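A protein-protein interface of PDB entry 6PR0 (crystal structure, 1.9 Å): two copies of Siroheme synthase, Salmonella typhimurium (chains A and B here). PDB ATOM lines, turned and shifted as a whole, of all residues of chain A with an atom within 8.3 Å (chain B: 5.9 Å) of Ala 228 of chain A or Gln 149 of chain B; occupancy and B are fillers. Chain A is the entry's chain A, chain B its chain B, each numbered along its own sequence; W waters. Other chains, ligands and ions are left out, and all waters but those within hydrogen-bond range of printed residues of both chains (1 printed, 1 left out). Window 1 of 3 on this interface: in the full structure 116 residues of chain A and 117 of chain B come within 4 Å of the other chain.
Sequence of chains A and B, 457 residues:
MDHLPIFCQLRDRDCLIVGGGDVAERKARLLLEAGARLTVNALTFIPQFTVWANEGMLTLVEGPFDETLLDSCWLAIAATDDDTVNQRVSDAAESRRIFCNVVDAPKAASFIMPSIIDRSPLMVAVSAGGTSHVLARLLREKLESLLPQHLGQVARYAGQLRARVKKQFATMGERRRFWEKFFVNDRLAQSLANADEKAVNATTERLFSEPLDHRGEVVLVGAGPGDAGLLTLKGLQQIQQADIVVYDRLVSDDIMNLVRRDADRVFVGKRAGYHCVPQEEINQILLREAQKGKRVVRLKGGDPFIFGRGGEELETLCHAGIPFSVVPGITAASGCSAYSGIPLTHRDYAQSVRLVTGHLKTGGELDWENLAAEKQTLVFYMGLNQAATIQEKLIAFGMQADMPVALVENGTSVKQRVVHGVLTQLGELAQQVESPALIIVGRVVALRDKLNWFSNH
The backbone NH (N) of Leu 233 of chain B sits at hydrogen-bond distance from the backbone carbonyl oxygen (O) of Gly 229 of chain A, at 3.3 Å.
N of Leu 233 of chain B sits at hydrogen-bond distance from O of Leu 231 of chain A (2.9 Å).
The backbone NH (N) of Gly 229 of chain A is in hydrogen-bond range of the side-chain carboxylate (OD1) of Asp 227 of chain A.
The guanidinium group (NH2) of Arg 119 of chain B is in salt-bridge range of the side-chain carboxylate (OE1) of Glu 144 of chain B (2.8 Å).
NH2 of Arg 119 of chain B sits close to NE2 of Gln 149 of chain B (3.4 Å).
O of Leu 233 of chain B lies close to NE2 of Gln 237 of chain B, at 3.4 Å.
OE1 of Gln 149 of chain B touches CB of Ala 228 of chain A, 3.6 Å away.
Leu 233 of chain B touches Ala 228 of chain A (CD1 to O, 3.8 Å).
Gly 229 of chain A touches Gln 149 of chain B.
Thr 232 of chain A touches Leu 233 of chain B.
Leu 233 of chain B touches Leu 233 of chain A.
Leu 236 of chain A touches Leu 233 of chain B.
OE1 of Glu 144 of chain B touches CD2 of Leu 258 of chain A (3.4 Å).
Of chain B, only Gln 149 and Leu 233 come within 4 Å of Ala 228 of chain A.
Printed residues of chain B within 4 Å of Gly 229 of chain A: Gln 149 and Leu 233.
Printed residues of chain B within 4 Å of Leu 231 of chain A: Leu 233.
Of the printed residues of chain B, Leu 236 of chain A touches Leu 233 (3.9 Å).
Ser 252 of chain A touches none of the printed residues of chain B.
Of the printed residues of chain B, Leu 258 of chain A touches Glu 144.
Leu 147 of chain B touches none of the printed residues of chain A.
Of chain A, only Ala 228 and Gly 229 come within 4 Å of Gln 149 of chain B.
Of the printed residues of chain A, Leu 233 of chain B touches Ala 228, Gly 229, Leu 231, Thr 232, Leu 233 and Leu 236.
The nearest printed residue of chain B that does not touch Ala 228 of chain A is His 150 of chain B (6.6 Å).
The nearest residue of chain A that does not touch Gln 149 of chain B is Leu 258 of chain A (4.1 Å).
The nearest printed residue of chain B that does not touch Thr 232 of chain A is Glu 144 of chain B (9.1 Å).
Printed residues of chain A that touch a printed residue of chain B: Ala 228, Gly 229, Leu 231, Thr 232, Leu 233, Leu 236 and Leu 258.
Hydrophobic or aromatic side chains of chain A within 4 Å of the printed part of chain B: Ala 228, Leu 233, Leu 236 and Leu 258.
Hydrophobic or aromatic side chains of chain B that line the printed part of chain A: Leu 233.
Leu 233 of chain A touches its own counterpart, Leu 233 of chain B.
Position printed for both chains: 233.
Water W1 bridges OE1 of Gln 149 of chain B and O of Asp 254 of chain A.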
ATOM      1  N   ALA A 223      -5.202 -23.454  29.063  1.00  0.00           N
ATOM      2  CA  ALA A 223      -5.397 -22.114  28.509  1.00  0.00           C
ATOM      3  C   ALA A 223      -6.687 -21.459  28.992  1.00  0.00           C
ATOM      4  O   ALA A 223      -6.830 -20.231  28.885  1.00  0.00           O
ATOM      5  CB  ALA A 223      -5.420 -22.186  26.979  1.00  0.00           C
ATOM      6  N   GLY A 224      -7.615 -22.236  29.543  1.00  0.00           N
ATOM      7  CA  GLY A 224      -8.941 -21.729  29.819  1.00  0.00           C
ATOM      8  C   GLY A 224      -9.791 -21.763  28.561  1.00  0.00           C
ATOM      9  O   GLY A 224      -9.332 -22.185  27.508  1.00  0.00           O
ATOM     10  N   PRO A 225     -11.048 -21.305  28.640  1.00  0.00           N
ATOM     11  CA  PRO A 225     -11.966 -21.510  27.513  1.00  0.00           C
ATOM     12  C   PRO A 225     -11.840 -20.487  26.398  1.00  0.00           C
ATOM     13  O   PRO A 225     -12.443 -20.686  25.338  1.00  0.00           O
ATOM     14  CB  PRO A 225     -13.363 -21.461  28.176  1.00  0.00           C
ATOM     15  CG  PRO A 225     -13.177 -20.733  29.420  1.00  0.00           C
ATOM     16  CD  PRO A 225     -11.705 -20.721  29.813  1.00  0.00           C
ATOM     17  N   GLY A 226     -11.091 -19.411  26.574  1.00  0.00           N
ATOM     18  CA  GLY A 226     -10.882 -18.521  25.442  1.00  0.00           C
ATOM     19  C   GLY A 226     -10.405 -17.127  25.809  1.00  0.00           C
ATOM     20  O   GLY A 226      -9.394 -16.667  25.263  1.00  0.00           O
ATOM     21  N   ASP A 227     -11.134 -16.447  26.699  1.00  0.00           N
ATOM     22  CA  ASP A 227     -10.736 -15.139  27.218  1.00  0.00           C
ATOM     23  C   ASP A 227      -9.310 -15.203  27.771  1.00  0.00           C
ATOM     24  O   ASP A 227      -9.043 -15.945  28.722  1.00  0.00           O
ATOM     25  CB  ASP A 227     -11.743 -14.729  28.309  1.00  0.00           C
ATOM     26  CG  ASP A 227     -11.523 -13.304  28.860  1.00  0.00           C
ATOM     27  OD1 ASP A 227     -10.433 -12.702  28.704  1.00  0.00           O
ATOM     28  OD2 ASP A 227     -12.469 -12.786  29.492  1.00  0.00           O
ATOM     29  N   ALA A 228      -8.384 -14.449  27.166  1.00  0.00           N
ATOM     30  CA  ALA A 228      -6.988 -14.515  27.611  1.00  0.00           C
ATOM     31  C   ALA A 228      -6.836 -14.077  29.064  1.00  0.00           C
ATOM     32  O   ALA A 228      -5.917 -14.529  29.754  1.00  0.00           O
ATOM     33  CB  ALA A 228      -6.083 -13.658  26.705  1.00  0.00           C
ATOM     34  N   GLY A 229      -7.738 -13.214  29.548  1.00  0.00           N
ATOM     35  CA  GLY A 229      -7.777 -12.840  30.949  1.00  0.00           C
ATOM     36  C   GLY A 229      -7.987 -14.004  31.901  1.00  0.00           C
ATOM     37  O   GLY A 229      -7.736 -13.857  33.102  1.00  0.00           O
ATOM     38  N   LEU A 230      -8.447 -15.161  31.405  1.00  0.00           N
ATOM     39  CA  LEU A 230      -8.667 -16.323  32.269  1.00  0.00           C
ATOM     40  C   LEU A 230      -7.477 -17.290  32.294  1.00  0.00           C
ATOM     41  O   LEU A 230      -7.555 -18.331  32.946  1.00  0.00           O
ATOM     42  CB  LEU A 230      -9.940 -17.087  31.850  1.00  0.00           C
ATOM     43  CG  LEU A 230     -11.239 -16.267  31.902  1.00  0.00           C
ATOM     44  CD1 LEU A 230     -12.478 -17.095  31.456  1.00  0.00           C
ATOM     45  CD2 LEU A 230     -11.454 -15.641  33.282  1.00  0.00           C
ATOM     46  N   LEU A 231      -6.371 -16.972  31.625  1.00  0.00           N
ATOM     47  CA  LEU A 231      -5.164 -17.743  31.877  1.00  0.00           C
ATOM     48  C   LEU A 231      -4.733 -17.497  33.324  1.00  0.00           C
ATOM     49  O   LEU A 231      -4.968 -16.421  33.880  1.00  0.00           O
ATOM     50  CB  LEU A 231      -4.076 -17.329  30.885  1.00  0.00           C
ATOM     51  CG  LEU A 231      -2.722 -18.041  30.836  1.00  0.00           C
ATOM     52  CD1 LEU A 231      -2.871 -19.494  30.406  1.00  0.00           C
ATOM     53  CD2 LEU A 231      -1.766 -17.284  29.882  1.00  0.00           C
ATOM     54  N   THR A 232      -4.109 -18.498  33.941  1.00  0.00           N
ATOM     55  CA  THR A 232      -3.554 -18.313  35.279  1.00  0.00           C
ATOM     56  C   THR A 232      -2.204 -17.596  35.193  1.00  0.00           C
ATOM     57  O   THR A 232      -1.546 -17.605  34.159  1.00  0.00           O
ATOM     58  CB  THR A 232      -3.361 -19.660  35.981  1.00  0.00           C
ATOM     59  OG1 THR A 232      -2.448 -20.473  35.217  1.00  0.00           O
ATOM     60  CG2 THR A 232      -4.712 -20.375  36.129  1.00  0.00           C
ATOM     61  N   LEU A 233      -1.800 -16.968  36.307  1.00  0.00           N
ATOM     62  CA  LEU A 233      -0.490 -16.330  36.360  1.00  0.00           C
ATOM     63  C   LEU A 233       0.616 -17.344  36.099  1.00  0.00           C
ATOM     64  O   LEU A 233       1.615 -17.031  35.448  1.00  0.00           O
ATOM     65  CB  LEU A 233      -0.280 -15.669  37.724  1.00  0.00           C
ATOM     66  CG  LEU A 233      -1.286 -14.562  38.005  1.00  0.00           C
ATOM     67  CD1 LEU A 233      -1.284 -14.141  39.478  1.00  0.00           C
ATOM     68  CD2 LEU A 233      -0.918 -13.431  37.130  1.00  0.00           C
ATOM     69  N   LEU A 236       0.684 -18.227  32.373  1.00  0.00           N
ATOM     70  CA  LEU A 236       1.368 -17.167  31.638  1.00  0.00           C
ATOM     71  C   LEU A 236       2.868 -17.257  31.838  1.00  0.00           C
ATOM     72  O   LEU A 236       3.641 -17.081  30.888  1.00  0.00           O
ATOM     73  CB  LEU A 236       0.853 -15.795  32.079  1.00  0.00           C
ATOM     74  CG  LEU A 236       1.602 -14.570  31.519  1.00  0.00           C
ATOM     75  CD1 LEU A 236       1.370 -14.480  30.015  1.00  0.00           C
ATOM     76  CD2 LEU A 236       1.138 -13.271  32.206  1.00  0.00           C
ATOM     77  N   ILE A 239       4.112 -20.123  29.498  1.00  0.00           N
ATOM     78  CA  ILE A 239       4.204 -19.856  28.067  1.00  0.00           C
ATOM     79  C   ILE A 239       5.133 -18.681  27.756  1.00  0.00           C
ATOM     80  O   ILE A 239       5.640 -18.594  26.639  1.00  0.00           O
ATOM     81  CB  ILE A 239       2.834 -19.618  27.421  1.00  0.00           C
ATOM     82  CG1 ILE A 239       2.147 -18.384  27.989  1.00  0.00           C
ATOM     83  CG2 ILE A 239       1.921 -20.868  27.560  1.00  0.00           C
ATOM     84  CD1 ILE A 239       0.808 -18.163  27.349  1.00  0.00           C
ATOM     85  N   SER A 252      -7.253 -20.044  22.135  1.00  0.00           N
ATOM     86  CA  SER A 252      -7.669 -18.845  21.418  1.00  0.00           C
ATOM     87  C   SER A 252      -6.466 -18.077  20.878  1.00  0.00           C
ATOM     88  O   SER A 252      -5.340 -18.199  21.365  1.00  0.00           O
ATOM     89  CB  SER A 252      -8.490 -17.938  22.334  1.00  0.00           C
ATOM     90  OG  SER A 252      -7.680 -17.427  23.382  1.00  0.00           O
ATOM     91  N   ASP A 253      -6.728 -17.261  19.851  1.00  0.00           N
ATOM     92  CA  ASP A 253      -5.671 -16.424  19.284  1.00  0.00           C
ATOM     93  C   ASP A 253      -5.118 -15.456  20.321  1.00  0.00           C
ATOM     94  O   ASP A 253      -3.918 -15.153  20.318  1.00  0.00           O
ATOM     95  CB  ASP A 253      -6.196 -15.651  18.081  1.00  0.00           C
ATOM     96  CG  ASP A 253      -6.436 -16.538  16.880  1.00  0.00           C
ATOM     97  OD1 ASP A 253      -5.902 -17.669  16.855  1.00  0.00           O
ATOM     98  OD2 ASP A 253      -7.149 -16.097  15.955  1.00  0.00           O
ATOM     99  N   ASP A 254      -5.981 -14.951  21.213  1.00  0.00           N
ATOM    100  CA  ASP A 254      -5.520 -14.012  22.231  1.00  0.00           C
ATOM    101  C   ASP A 254      -4.538 -14.675  23.184  1.00  0.00           C
ATOM    102  O   ASP A 254      -3.577 -14.046  23.634  1.00  0.00           O
ATOM    103  CB  ASP A 254      -6.703 -13.439  23.011  1.00  0.00           C
ATOM    104  CG  ASP A 254      -7.482 -12.412  22.208  1.00  0.00           C
ATOM    105  OD1 ASP A 254      -6.945 -11.921  21.188  1.00  0.00           O
ATOM    106  OD2 ASP A 254      -8.620 -12.087  22.608  1.00  0.00           O
ATOM    107  N   ILE A 255      -4.768 -15.942  23.516  1.00  0.00           N
ATOM    108  CA  ILE A 255      -3.835 -16.633  24.402  1.00  0.00           C
ATOM    109  C   ILE A 255      -2.525 -16.892  23.678  1.00  0.00           C
ATOM    110  O   ILE A 255      -1.439 -16.656  24.230  1.00  0.00           O
ATOM    111  CB  ILE A 255      -4.471 -17.923  24.950  1.00  0.00           C
ATOM    112  CG1 ILE A 255      -5.393 -17.565  26.112  1.00  0.00           C
ATOM    113  CG2 ILE A 255      -3.393 -18.936  25.402  1.00  0.00           C
ATOM    114  CD1 ILE A 255      -6.436 -18.572  26.361  1.00  0.00           C
ATOM    115  N   MET A 256      -2.605 -17.314  22.407  1.00  0.00           N
ATOM    116  CA  MET A 256      -1.395 -17.502  21.612  1.00  0.00           C
ATOM    117  C   MET A 256      -0.582 -16.219  21.499  1.00  0.00           C
ATOM    118  O   MET A 256       0.646 -16.278  21.362  1.00  0.00           O
ATOM    119  CB  MET A 256      -1.747 -18.035  20.224  1.00  0.00           C
ATOM    120  CG  MET A 256      -2.232 -19.484  20.246  1.00  0.00           C
ATOM    121  SD  MET A 256      -1.126 -20.603  21.138  1.00  0.00           S
ATOM    122  CE  MET A 256       0.368 -20.442  20.122  1.00  0.00           C
ATOM    123  N   ASN A 257      -1.228 -15.053  21.560  1.00  0.00           N
ATOM    124  CA  ASN A 257      -0.442 -13.825  21.517  1.00  0.00           C
ATOM    125  C   ASN A 257       0.332 -13.585  22.805  1.00  0.00           C
ATOM    126  O   ASN A 257       1.156 -12.668  22.849  1.00  0.00           O
ATOM    127  CB  ASN A 257      -1.335 -12.617  21.222  1.00  0.00           C
ATOM    128  CG  ASN A 257      -1.824 -12.595  19.786  1.00  0.00           C
ATOM    129  OD1 ASN A 257      -1.295 -13.303  18.927  1.00  0.00           O
ATOM    130  ND2 ASN A 257      -2.838 -11.782  19.520  1.00  0.00           N
ATOM    131  N   LEU A 258       0.094 -14.383  23.848  1.00  0.00           N
ATOM    132  CA  LEU A 258       0.844 -14.273  25.090  1.00  0.00           C
ATOM    133  C   LEU A 258       2.039 -15.225  25.140  1.00  0.00           C
ATOM    134  O   LEU A 258       2.779 -15.229  26.127  1.00  0.00           O
ATOM    135  CB  LEU A 258      -0.086 -14.522  26.279  1.00  0.00           C
ATOM    136  CG  LEU A 258      -1.186 -13.465  26.393  1.00  0.00           C
ATOM    137  CD1 LEU A 258      -2.090 -13.766  27.559  1.00  0.00           C
ATOM    138  CD2 LEU A 258      -0.555 -12.092  26.547  1.00  0.00           C
ATOM    139  N   TYR A 339     -19.826 -16.607  32.554  1.00  0.00           N
ATOM    140  CA  TYR A 339     -20.073 -15.613  31.516  1.00  0.00           C
ATOM    141  C   TYR A 339     -21.469 -15.700  30.915  1.00  0.00           C
ATOM    142  O   TYR A 339     -21.865 -14.782  30.176  1.00  0.00           O
ATOM    143  CB  TYR A 339     -19.041 -15.740  30.396  1.00  0.00           C
ATOM    144  CG  TYR A 339     -17.673 -15.184  30.742  1.00  0.00           C
ATOM    145  CD1 TYR A 339     -16.955 -15.655  31.834  1.00  0.00           C
ATOM    146  CD2 TYR A 339     -17.094 -14.184  29.967  1.00  0.00           C
ATOM    147  CE1 TYR A 339     -15.699 -15.153  32.142  1.00  0.00           C
ATOM    148  CE2 TYR A 339     -15.841 -13.666  30.274  1.00  0.00           C
ATOM    149  CZ  TYR A 339     -15.146 -14.161  31.351  1.00  0.00           C
ATOM    150  OH  TYR A 339     -13.893 -13.653  31.645  1.00  0.00           O
ATOM    151  N   THR A 412     -17.036 -17.211  26.931  1.00  0.00           N
ATOM    152  CA  THR A 412     -16.029 -16.253  27.432  1.00  0.00           C
ATOM    153  C   THR A 412     -15.352 -15.446  26.328  1.00  0.00           C
ATOM    154  O   THR A 412     -14.613 -14.492  26.623  1.00  0.00           O
ATOM    155  CB  THR A 412     -14.947 -16.902  28.322  1.00  0.00           C
ATOM    156  OG1 THR A 412     -13.855 -17.450  27.540  1.00  0.00           O
ATOM    157  CG2 THR A 412     -15.539 -17.988  29.280  1.00  0.00           C
ATOM    158  N   SER A 413     -15.593 -15.768  25.063  1.00  0.00           N
ATOM    159  CA  SER A 413     -14.984 -14.949  24.018  1.00  0.00           C
ATOM    160  C   SER A 413     -15.898 -13.780  23.651  1.00  0.00           C
ATOM    161  O   SER A 413     -17.095 -13.777  23.947  1.00  0.00           O
ATOM    162  CB  SER A 413     -14.680 -15.781  22.782  1.00  0.00           C
ATOM    163  OG  SER A 413     -15.786 -15.780  21.914  1.00  0.00           O
ATOM    164  N   VAL A 414     -15.321 -12.771  22.995  1.00  0.00           N
ATOM    165  CA  VAL A 414     -16.137 -11.653  22.524  1.00  0.00           C
ATOM    166  C   VAL A 414     -17.197 -12.084  21.510  1.00  0.00           C
ATOM    167  O   VAL A 414     -18.121 -11.313  21.235  1.00  0.00           O
ATOM    168  CB  VAL A 414     -15.267 -10.524  21.921  1.00  0.00           C
ATOM    169  CG1 VAL A 414     -14.170 -10.048  22.912  1.00  0.00           C
ATOM    170  CG2 VAL A 414     -14.662 -10.945  20.592  1.00  0.00           C
ATOM    171  N   ASP B 118       1.499  -5.391  23.598  1.00  0.00           N
ATOM    172  CA  ASP B 118       0.632  -4.751  22.603  1.00  0.00           C
ATOM    173  C   ASP B 118      -0.779  -4.624  23.170  1.00  0.00           C
ATOM    174  O   ASP B 118      -1.460  -5.630  23.384  1.00  0.00           O
ATOM    175  CB  ASP B 118       0.623  -5.567  21.307  1.00  0.00           C
ATOM    176  CG  ASP B 118      -0.259  -4.954  20.209  1.00  0.00           C
ATOM    177  OD1 ASP B 118      -0.705  -3.799  20.354  1.00  0.00           O
ATOM    178  OD2 ASP B 118      -0.486  -5.632  19.180  1.00  0.00           O
ATOM    179  N   ARG B 119      -1.225  -3.391  23.380  1.00  0.00           N
ATOM    180  CA  ARG B 119      -2.629  -3.085  23.643  1.00  0.00           C
ATOM    181  C   ARG B 119      -3.082  -1.963  22.711  1.00  0.00           C
ATOM    182  O   ARG B 119      -3.680  -0.970  23.134  1.00  0.00           O
ATOM    183  CB  ARG B 119      -2.837  -2.711  25.115  1.00  0.00           C
ATOM    184  CG  ARG B 119      -2.386  -3.814  26.113  1.00  0.00           C
ATOM    185  CD  ARG B 119      -3.385  -4.989  26.209  1.00  0.00           C
ATOM    186  NE  ARG B 119      -3.000  -5.886  27.296  1.00  0.00           N
ATOM    187  CZ  ARG B 119      -2.048  -6.813  27.188  1.00  0.00           C
ATOM    188  NH1 ARG B 119      -1.402  -6.982  26.031  1.00  0.00           N
ATOM    189  NH2 ARG B 119      -1.744  -7.580  28.230  1.00  0.00           N
ATOM    190  N   GLU B 144       2.407  -8.017  31.017  1.00  0.00           N
ATOM    191  CA  GLU B 144       1.277  -8.653  30.344  1.00  0.00           C
ATOM    192  C   GLU B 144       0.218  -9.066  31.350  1.00  0.00           C
ATOM    193  O   GLU B 144      -0.976  -9.032  31.043  1.00  0.00           O
ATOM    194  CB  GLU B 144       1.728  -9.872  29.545  1.00  0.00           C
ATOM    195  CG  GLU B 144       2.558  -9.538  28.325  1.00  0.00           C
ATOM    196  CD  GLU B 144       1.722  -9.194  27.107  1.00  0.00           C
ATOM    197  OE1 GLU B 144       0.488  -8.962  27.250  1.00  0.00           O
ATOM    198  OE2 GLU B 144       2.316  -9.160  26.005  1.00  0.00           O
ATOM    199  N   LEU B 147      -1.669  -5.513  32.534  1.00  0.00           N
ATOM    200  CA  LEU B 147      -2.437  -4.673  31.616  1.00  0.00           C
ATOM    201  C   LEU B 147      -3.642  -5.440  31.097  1.00  0.00           C
ATOM    202  O   LEU B 147      -3.461  -6.444  30.394  1.00  0.00           O
ATOM    203  CB  LEU B 147      -1.579  -4.223  30.450  1.00  0.00           C
ATOM    204  CG  LEU B 147      -0.429  -3.284  30.830  1.00  0.00           C
ATOM    205  CD1 LEU B 147       0.358  -2.920  29.571  1.00  0.00           C
ATOM    206  CD2 LEU B 147      -0.983  -2.031  31.496  1.00  0.00           C
ATOM    207  N   PRO B 148      -4.872  -4.997  31.386  1.00  0.00           N
ATOM    208  CA  PRO B 148      -6.048  -5.735  30.916  1.00  0.00           C
ATOM    209  C   PRO B 148      -6.035  -5.890  29.412  1.00  0.00           C
ATOM    210  O   PRO B 148      -5.518  -5.044  28.680  1.00  0.00           O
ATOM    211  CB  PRO B 148      -7.235  -4.872  31.381  1.00  0.00           C
ATOM    212  CG  PRO B 148      -6.710  -4.185  32.598  1.00  0.00           C
ATOM    213  CD  PRO B 148      -5.239  -3.886  32.276  1.00  0.00           C
ATOM    214  N   GLN B 149      -6.584  -7.018  28.969  1.00  0.00           N
ATOM    215  CA  GLN B 149      -6.525  -7.396  27.564  1.00  0.00           C
ATOM    216  C   GLN B 149      -7.190  -6.368  26.657  1.00  0.00           C
ATOM    217  O   GLN B 149      -6.767  -6.199  25.512  1.00  0.00           O
ATOM    218  CB  GLN B 149      -7.196  -8.753  27.382  1.00  0.00           C
ATOM    219  CG  GLN B 149      -6.369  -9.905  27.910  1.00  0.00           C
ATOM    220  CD  GLN B 149      -5.101 -10.102  27.094  1.00  0.00           C
ATOM    221  OE1 GLN B 149      -5.155 -10.248  25.873  1.00  0.00           O
ATOM    222  NE2 GLN B 149      -3.950 -10.078  27.768  1.00  0.00           N
ATOM    223  N   HIS B 150      -8.239  -5.690  27.127  1.00  0.00           N
ATOM    224  CA  HIS B 150      -8.993  -4.787  26.262  1.00  0.00           C
ATOM    225  C   HIS B 150      -8.720  -3.316  26.556  1.00  0.00           C
ATOM    226  O   HIS B 150      -9.523  -2.449  26.191  1.00  0.00           O
ATOM    227  CB  HIS B 150     -10.480  -5.127  26.363  1.00  0.00           C
ATOM    228  CG  HIS B 150     -10.751  -6.552  26.002  1.00  0.00           C
ATOM    229  ND1 HIS B 150     -10.389  -7.080  24.781  1.00  0.00           N
ATOM    230  CD2 HIS B 150     -11.270  -7.576  26.717  1.00  0.00           C
ATOM    231  CE1 HIS B 150     -10.697  -8.363  24.751  1.00  0.00           C
ATOM    232  NE2 HIS B 150     -11.243  -8.685  25.908  1.00  0.00           N
ATOM    233  N   LEU B 151      -7.589  -3.020  27.197  1.00  0.00           N
ATOM    234  CA  LEU B 151      -7.249  -1.636  27.495  1.00  0.00           C
ATOM    235  C   LEU B 151      -7.203  -0.783  26.235  1.00  0.00           C
ATOM    236  O   LEU B 151      -7.536   0.398  26.282  1.00  0.00           O
ATOM    237  CB  LEU B 151      -5.907  -1.580  28.214  1.00  0.00           C
ATOM    238  CG  LEU B 151      -5.548  -0.274  28.914  1.00  0.00           C
ATOM    239  CD1 LEU B 151      -6.649   0.169  29.827  1.00  0.00           C
ATOM    240  CD2 LEU B 151      -4.267  -0.472  29.712  1.00  0.00           C
ATOM    241  N   GLY B 152      -6.792  -1.356  25.104  1.00  0.00           N
ATOM    242  CA  GLY B 152      -6.703  -0.568  23.891  1.00  0.00           C
ATOM    243  C   GLY B 152      -8.049  -0.074  23.410  1.00  0.00           C
ATOM    244  O   GLY B 152      -8.145   1.030  22.867  1.00  0.00           O
ATOM    245  N   LEU B 233      -5.294 -13.891  35.301  1.00  0.00           N
ATOM    246  CA  LEU B 233      -4.825 -12.534  35.022  1.00  0.00           C
ATOM    247  C   LEU B 233      -5.896 -11.507  35.356  1.00  0.00           C
ATOM    248  O   LEU B 233      -5.615 -10.463  35.962  1.00  0.00           O
ATOM    249  CB  LEU B 233      -4.416 -12.380  33.554  1.00  0.00           C
ATOM    250  CG  LEU B 233      -3.497 -13.455  32.941  1.00  0.00           C
ATOM    251  CD1 LEU B 233      -2.979 -13.006  31.577  1.00  0.00           C
ATOM    252  CD2 LEU B 233      -2.372 -13.783  33.906  1.00  0.00           C
ATOM    253  N   GLN B 237      -5.897  -8.366  38.110  1.00  0.00           N
ATOM    254  CA  GLN B 237      -6.186  -6.990  37.720  1.00  0.00           C
ATOM    255  C   GLN B 237      -7.311  -6.400  38.566  1.00  0.00           C
ATOM    256  O   GLN B 237      -7.253  -5.238  38.995  1.00  0.00           O
ATOM    257  CB  GLN B 237      -6.554  -6.966  36.240  1.00  0.00           C
ATOM    258  CG  GLN B 237      -5.382  -7.361  35.356  1.00  0.00           C
ATOM    259  CD  GLN B 237      -5.783  -7.916  34.001  1.00  0.00           C
ATOM    260  OE1 GLN B 237      -6.942  -7.830  33.570  1.00  0.00           O
ATOM    261  NE2 GLN B 237      -4.804  -8.485  33.305  1.00  0.00           N
HETATM  262  O   HOH W   1      -3.501 -11.183  24.077  1.00  0.00           O
